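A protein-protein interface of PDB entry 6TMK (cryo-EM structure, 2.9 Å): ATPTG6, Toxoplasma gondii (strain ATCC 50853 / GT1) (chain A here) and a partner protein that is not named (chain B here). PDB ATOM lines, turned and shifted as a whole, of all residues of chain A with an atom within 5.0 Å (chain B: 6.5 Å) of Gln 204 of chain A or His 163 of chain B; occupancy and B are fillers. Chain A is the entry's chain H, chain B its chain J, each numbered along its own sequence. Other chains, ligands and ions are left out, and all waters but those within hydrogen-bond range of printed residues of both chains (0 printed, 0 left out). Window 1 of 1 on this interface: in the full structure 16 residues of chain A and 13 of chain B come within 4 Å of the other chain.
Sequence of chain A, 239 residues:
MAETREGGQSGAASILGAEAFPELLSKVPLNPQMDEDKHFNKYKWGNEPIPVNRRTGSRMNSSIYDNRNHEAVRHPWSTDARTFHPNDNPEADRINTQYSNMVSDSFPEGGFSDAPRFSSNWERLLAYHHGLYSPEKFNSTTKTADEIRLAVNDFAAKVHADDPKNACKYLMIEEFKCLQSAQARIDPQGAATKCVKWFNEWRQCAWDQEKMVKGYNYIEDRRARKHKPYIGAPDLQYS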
ATOM      1  N   ASN A 200      12.682  -6.895   5.139  1.00  0.00           N
ATOM      2  CA  ASN A 200      13.788  -6.150   5.726  1.00  0.00           C
ATOM      3  C   ASN A 200      13.312  -4.849   6.370  1.00  0.00           C
ATOM      4  O   ASN A 200      13.776  -4.475   7.456  1.00  0.00           O
ATOM      5  CB  ASN A 200      14.830  -5.885   4.643  1.00  0.00           C
ATOM      6  CG  ASN A 200      16.089  -5.263   5.175  1.00  0.00           C
ATOM      7  OD1 ASN A 200      16.672  -5.730   6.153  1.00  0.00           O
ATOM      8  ND2 ASN A 200      16.525  -4.198   4.526  1.00  0.00           N
ATOM      9  N   GLU A 201      12.380  -4.148   5.723  1.00  0.00           N
ATOM     10  CA  GLU A 201      11.855  -2.920   6.311  1.00  0.00           C
ATOM     11  C   GLU A 201      11.097  -3.203   7.603  1.00  0.00           C
ATOM     12  O   GLU A 201      11.197  -2.440   8.571  1.00  0.00           O
ATOM     13  CB  GLU A 201      10.946  -2.205   5.318  1.00  0.00           C
ATOM     14  CG  GLU A 201      11.642  -1.591   4.138  1.00  0.00           C
ATOM     15  CD  GLU A 201      12.467  -0.374   4.494  1.00  0.00           C
ATOM     16  OE1 GLU A 201      11.946   0.518   5.197  1.00  0.00           O
ATOM     17  OE2 GLU A 201      13.639  -0.304   4.069  1.00  0.00           O
ATOM     18  N   TRP A 202      10.331  -4.296   7.638  1.00  0.00           N
ATOM     19  CA  TRP A 202       9.665  -4.701   8.870  1.00  0.00           C
ATOM     20  C   TRP A 202      10.677  -5.023   9.963  1.00  0.00           C
ATOM     21  O   TRP A 202      10.484  -4.668  11.132  1.00  0.00           O
ATOM     22  CB  TRP A 202       8.750  -5.895   8.591  1.00  0.00           C
ATOM     23  CG  TRP A 202       8.236  -6.571   9.808  1.00  0.00           C
ATOM     24  CD1 TRP A 202       7.078  -6.297  10.455  1.00  0.00           C
ATOM     25  CD2 TRP A 202       8.848  -7.646  10.522  1.00  0.00           C
ATOM     26  NE1 TRP A 202       6.931  -7.119  11.535  1.00  0.00           N
ATOM     27  CE2 TRP A 202       8.007  -7.959  11.600  1.00  0.00           C
ATOM     28  CE3 TRP A 202      10.030  -8.370  10.361  1.00  0.00           C
ATOM     29  CZ2 TRP A 202       8.305  -8.963  12.505  1.00  0.00           C
ATOM     30  CZ3 TRP A 202      10.320  -9.362  11.263  1.00  0.00           C
ATOM     31  CH2 TRP A 202       9.462  -9.651  12.319  1.00  0.00           C
ATOM     32  N   ARG A 203      11.754  -5.712   9.594  1.00  0.00           N
ATOM     33  CA  ARG A 203      12.824  -6.030  10.531  1.00  0.00           C
ATOM     34  C   ARG A 203      13.426  -4.767  11.132  1.00  0.00           C
ATOM     35  O   ARG A 203      13.771  -4.738  12.317  1.00  0.00           O
ATOM     36  CB  ARG A 203      13.885  -6.850   9.802  1.00  0.00           C
ATOM     37  CG  ARG A 203      14.685  -7.779  10.645  1.00  0.00           C
ATOM     38  CD  ARG A 203      15.422  -8.781   9.782  1.00  0.00           C
ATOM     39  NE  ARG A 203      16.400  -9.541  10.548  1.00  0.00           N
ATOM     40  CZ  ARG A 203      17.643  -9.144  10.791  1.00  0.00           C
ATOM     41  NH1 ARG A 203      18.079  -7.985  10.331  1.00  0.00           N
ATOM     42  NH2 ARG A 203      18.449  -9.909  11.506  1.00  0.00           N
ATOM     43  N   GLN A 204      13.582  -3.725  10.321  1.00  0.00           N
ATOM     44  CA  GLN A 204      14.089  -2.453  10.827  1.00  0.00           C
ATOM     45  C   GLN A 204      13.081  -1.782  11.753  1.00  0.00           C
ATOM     46  O   GLN A 204      13.442  -1.285  12.829  1.00  0.00           O
ATOM     47  CB  GLN A 204      14.436  -1.545   9.658  1.00  0.00           C
ATOM     48  CG  GLN A 204      15.558  -2.058   8.819  1.00  0.00           C
ATOM     49  CD  GLN A 204      15.780  -1.238   7.585  1.00  0.00           C
ATOM     50  OE1 GLN A 204      15.041  -0.302   7.300  1.00  0.00           O
ATOM     51  NE2 GLN A 204      16.813  -1.576   6.846  1.00  0.00           N
ATOM     52  N   CYS A 205      11.819  -1.720  11.329  1.00  0.00           N
ATOM     53  CA  CYS A 205      10.785  -1.085  12.136  1.00  0.00           C
ATOM     54  C   CYS A 205      10.651  -1.751  13.495  1.00  0.00           C
ATOM     55  O   CYS A 205      10.347  -1.082  14.489  1.00  0.00           O
ATOM     56  CB  CYS A 205       9.455  -1.111  11.387  1.00  0.00           C
ATOM     57  SG  CYS A 205       7.994  -0.823  12.397  1.00  0.00           S
ATOM     58  N   ALA A 206      10.884  -3.058  13.563  1.00  0.00           N
ATOM     59  CA  ALA A 206      10.796  -3.754  14.839  1.00  0.00           C
ATOM     60  C   ALA A 206      11.797  -3.191  15.836  1.00  0.00           C
ATOM     61  O   ALA A 206      11.453  -2.900  16.987  1.00  0.00           O
ATOM     62  CB  ALA A 206      11.023  -5.245  14.624  1.00  0.00           C
ATOM     63  N   TRP A 207      13.050  -3.043  15.417  1.00  0.00           N
ATOM     64  CA  TRP A 207      14.053  -2.470  16.301  1.00  0.00           C
ATOM     65  C   TRP A 207      13.773  -1.005  16.596  1.00  0.00           C
ATOM     66  O   TRP A 207      14.001  -0.545  17.718  1.00  0.00           O
ATOM     67  CB  TRP A 207      15.435  -2.637  15.680  1.00  0.00           C
ATOM     68  CG  TRP A 207      16.472  -1.763  16.284  1.00  0.00           C
ATOM     69  CD1 TRP A 207      17.117  -0.736  15.678  1.00  0.00           C
ATOM     70  CD2 TRP A 207      16.977  -1.820  17.616  1.00  0.00           C
ATOM     71  NE1 TRP A 207      17.994  -0.151  16.543  1.00  0.00           N
ATOM     72  CE2 TRP A 207      17.928  -0.800  17.744  1.00  0.00           C
ATOM     73  CE3 TRP A 207      16.721  -2.635  18.714  1.00  0.00           C
ATOM     74  CZ2 TRP A 207      18.621  -0.578  18.916  1.00  0.00           C
ATOM     75  CZ3 TRP A 207      17.413  -2.410  19.871  1.00  0.00           C
ATOM     76  CH2 TRP A 207      18.347  -1.392  19.966  1.00  0.00           C
ATOM     77  N   ASP A 208      13.310  -0.245  15.605  1.00  0.00           N
ATOM     78  CA  ASP A 208      13.012   1.159  15.864  1.00  0.00           C
ATOM     79  C   ASP A 208      11.909   1.318  16.905  1.00  0.00           C
ATOM     80  O   ASP A 208      12.000   2.180  17.797  1.00  0.00           O
ATOM     81  CB  ASP A 208      12.617   1.837  14.556  1.00  0.00           C
ATOM     82  CG  ASP A 208      13.748   1.872  13.552  1.00  0.00           C
ATOM     83  OD1 ASP A 208      14.916   1.733  13.963  1.00  0.00           O
ATOM     84  OD2 ASP A 208      13.463   2.030  12.348  1.00  0.00           O
ATOM     85  N   TYR B 152      30.173   0.873   6.097  1.00  0.00           N
ATOM     86  CA  TYR B 152      29.263   0.576   7.194  1.00  0.00           C
ATOM     87  C   TYR B 152      29.625   1.381   8.433  1.00  0.00           C
ATOM     88  O   TYR B 152      28.754   1.959   9.089  1.00  0.00           O
ATOM     89  CB  TYR B 152      29.282  -0.921   7.493  1.00  0.00           C
ATOM     90  CG  TYR B 152      28.149  -1.383   8.372  1.00  0.00           C
ATOM     91  CD1 TYR B 152      26.999  -1.920   7.831  1.00  0.00           C
ATOM     92  CD2 TYR B 152      28.238  -1.295   9.744  1.00  0.00           C
ATOM     93  CE1 TYR B 152      25.971  -2.341   8.628  1.00  0.00           C
ATOM     94  CE2 TYR B 152      27.212  -1.714  10.549  1.00  0.00           C
ATOM     95  CZ  TYR B 152      26.085  -2.238   9.991  1.00  0.00           C
ATOM     96  OH  TYR B 152      25.065  -2.655  10.806  1.00  0.00           O
ATOM     97  N   TYR B 156      27.360   4.179  10.268  1.00  0.00           N
ATOM     98  CA  TYR B 156      26.770   3.775  11.536  1.00  0.00           C
ATOM     99  C   TYR B 156      27.325   4.576  12.706  1.00  0.00           C
ATOM    100  O   TYR B 156      26.565   5.099  13.524  1.00  0.00           O
ATOM    101  CB  TYR B 156      27.015   2.283  11.784  1.00  0.00           C
ATOM    102  CG  TYR B 156      26.198   1.714  12.915  1.00  0.00           C
ATOM    103  CD1 TYR B 156      24.960   1.156  12.688  1.00  0.00           C
ATOM    104  CD2 TYR B 156      26.666   1.752  14.216  1.00  0.00           C
ATOM    105  CE1 TYR B 156      24.215   0.651  13.714  1.00  0.00           C
ATOM    106  CE2 TYR B 156      25.925   1.253  15.249  1.00  0.00           C
ATOM    107  CZ  TYR B 156      24.699   0.701  14.997  1.00  0.00           C
ATOM    108  OH  TYR B 156      23.961   0.201  16.040  1.00  0.00           O
ATOM    109  N   GLY B 160      25.176   8.176  12.415  1.00  0.00           N
ATOM    110  CA  GLY B 160      24.052   7.843  13.255  1.00  0.00           C
ATOM    111  C   GLY B 160      22.994   6.984  12.613  1.00  0.00           C
ATOM    112  O   GLY B 160      21.871   6.938  13.127  1.00  0.00           O
ATOM    113  N   LEU B 161      23.308   6.307  11.518  1.00  0.00           N
ATOM    114  CA  LEU B 161      22.346   5.466  10.826  1.00  0.00           C
ATOM    115  C   LEU B 161      22.387   4.064  11.412  1.00  0.00           C
ATOM    116  O   LEU B 161      23.427   3.402  11.378  1.00  0.00           O
ATOM    117  CB  LEU B 161      22.655   5.423   9.334  1.00  0.00           C
ATOM    118  CG  LEU B 161      22.793   6.768   8.627  1.00  0.00           C
ATOM    119  CD1 LEU B 161      23.075   6.542   7.174  1.00  0.00           C
ATOM    120  CD2 LEU B 161      21.549   7.595   8.795  1.00  0.00           C
ATOM    121  N   ASP B 162      21.250   3.608  11.927  1.00  0.00           N
ATOM    122  CA  ASP B 162      21.165   2.269  12.487  1.00  0.00           C
ATOM    123  C   ASP B 162      21.097   1.206  11.404  1.00  0.00           C
ATOM    124  O   ASP B 162      21.444   0.050  11.663  1.00  0.00           O
ATOM    125  CB  ASP B 162      19.953   2.165  13.406  1.00  0.00           C
ATOM    126  CG  ASP B 162      20.181   2.817  14.743  1.00  0.00           C
ATOM    127  OD1 ASP B 162      21.191   3.530  14.895  1.00  0.00           O
ATOM    128  OD2 ASP B 162      19.343   2.630  15.644  1.00  0.00           O
ATOM    129  N   HIS B 163      20.666   1.578  10.205  1.00  0.00           N
ATOM    130  CA  HIS B 163      20.489   0.658   9.087  1.00  0.00           C
ATOM    131  C   HIS B 163      21.224   1.223   7.883  1.00  0.00           C
ATOM    132  O   HIS B 163      20.611   1.786   6.965  1.00  0.00           O
ATOM    133  CB  HIS B 163      19.007   0.428   8.813  1.00  0.00           C
ATOM    134  CG  HIS B 163      18.237   0.047  10.032  1.00  0.00           C
ATOM    135  ND1 HIS B 163      18.415  -1.158  10.673  1.00  0.00           N
ATOM    136  CD2 HIS B 163      17.314   0.723  10.751  1.00  0.00           C
ATOM    137  CE1 HIS B 163      17.619  -1.215  11.723  1.00  0.00           C
ATOM    138  NE2 HIS B 163      16.941  -0.085  11.795  1.00  0.00           N
ATOM    139  N   PRO B 164      22.549   1.092   7.854  1.00  0.00           N
ATOM    140  CA  PRO B 164      23.330   1.759   6.808  1.00  0.00           C
ATOM    141  C   PRO B 164      23.199   1.112   5.446  1.00  0.00           C
ATOM    142  O   PRO B 164      23.307   1.808   4.432  1.00  0.00           O
ATOM    143  CB  PRO B 164      24.768   1.671   7.339  1.00  0.00           C
ATOM    144  CG  PRO B 164      24.672   1.071   8.683  1.00  0.00           C
ATOM    145  CD  PRO B 164      23.415   0.338   8.763  1.00  0.00           C
ATOM    146  N   PHE B 165      22.995  -0.196   5.392  1.00  0.00           N
ATOM    147  CA  PHE B 165      23.040  -0.958   4.157  1.00  0.00           C
ATOM    148  C   PHE B 165      21.630  -1.256   3.681  1.00  0.00           C
ATOM    149  O   PHE B 165      20.809  -1.783   4.438  1.00  0.00           O
ATOM    150  CB  PHE B 165      23.815  -2.261   4.350  1.00  0.00           C
ATOM    151  CG  PHE B 165      25.294  -2.127   4.172  1.00  0.00           C
ATOM    152  CD1 PHE B 165      25.890  -0.890   4.076  1.00  0.00           C
ATOM    153  CD2 PHE B 165      26.096  -3.246   4.119  1.00  0.00           C
ATOM    154  CE1 PHE B 165      27.235  -0.770   3.916  1.00  0.00           C
ATOM    155  CE2 PHE B 165      27.451  -3.126   3.964  1.00  0.00           C
ATOM    156  CZ  PHE B 165      28.021  -1.887   3.867  1.00  0.00           C
ATOM    157  N   THR B 166      21.353  -0.904   2.433  1.00  0.00           N
ATOM    158  CA  THR B 166      20.154  -1.365   1.763  1.00  0.00           C
ATOM    159  C   THR B 166      20.370  -2.779   1.236  1.00  0.00           C
ATOM    160  O   THR B 166      21.405  -3.415   1.460  1.00  0.00           O
ATOM    161  CB  THR B 166      19.759  -0.414   0.633  1.00  0.00           C
ATOM    162  OG1 THR B 166      20.689  -0.521  -0.451  1.00  0.00           O
ATOM    163  CG2 THR B 166      19.706   1.015   1.122  1.00  0.00           C
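OD2 of Asp 162 of chain B sits at hydrogen-bond distance from NE1 of Trp 207 of chain A, 3.2 Å away. NE2 of His 163 of chain B sits at hydrogen-bond distance from OD1 of Asp 208 of chain A, at 3.5 Å.
Of the 9 printed residues of chain B, 2 touch a printed residue of chain A. Printed residues of chain B that touch a printed residue of chain A: Asp 162 and His 163. Hydrophobic or aromatic side chains of chain B within 4 Å of the printed part of chain A: His 163. Along chain B the printed residues that touch a printed residue of chain A span positions 162 to 163. Of the 9 printed residues of chain A, 3 touch a printed residue of chain B. Hydrophobic or aromatic side chains of chain A within 4 Å of the printed part of chain B: Trp 207. Among the printed residues, no Asp or Glu carboxylate lies within 4 Å of a Lys or Arg side-chain nitrogen of the other chain.
Gln 204 of chain A touches one residue of chain B. Of the printed residues of chain A, Asp 162 of chain B touches Trp 207. Of the printed residues of chain B, Trp 207 of chain A touches Asp 162 and His 163. Of the printed residues of chain B, Asp 208 of chain A touches His 163 (3.5 Å). Pro 164 of chain B touches none of the printed residues of chain A. The nearest residue of chain B that does not touch Gln 204 of chain A is Phe 165 of chain B (4.7 Å). The nearest printed residue of chain A that does not touch His 163 of chain B is Arg 203 of chain A (5.3 Å). The nearest printed residue of chain A that does not touch Asp 162 of chain B is Asp 208 of chain A (4.8 Å).
Among the printed residues, merely in contact across the chains: Gln 204 of chain A with His 163 of chain B (3.5 Å) and Trp 207 of chain A with His 163 of chain B (3.9 Å).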
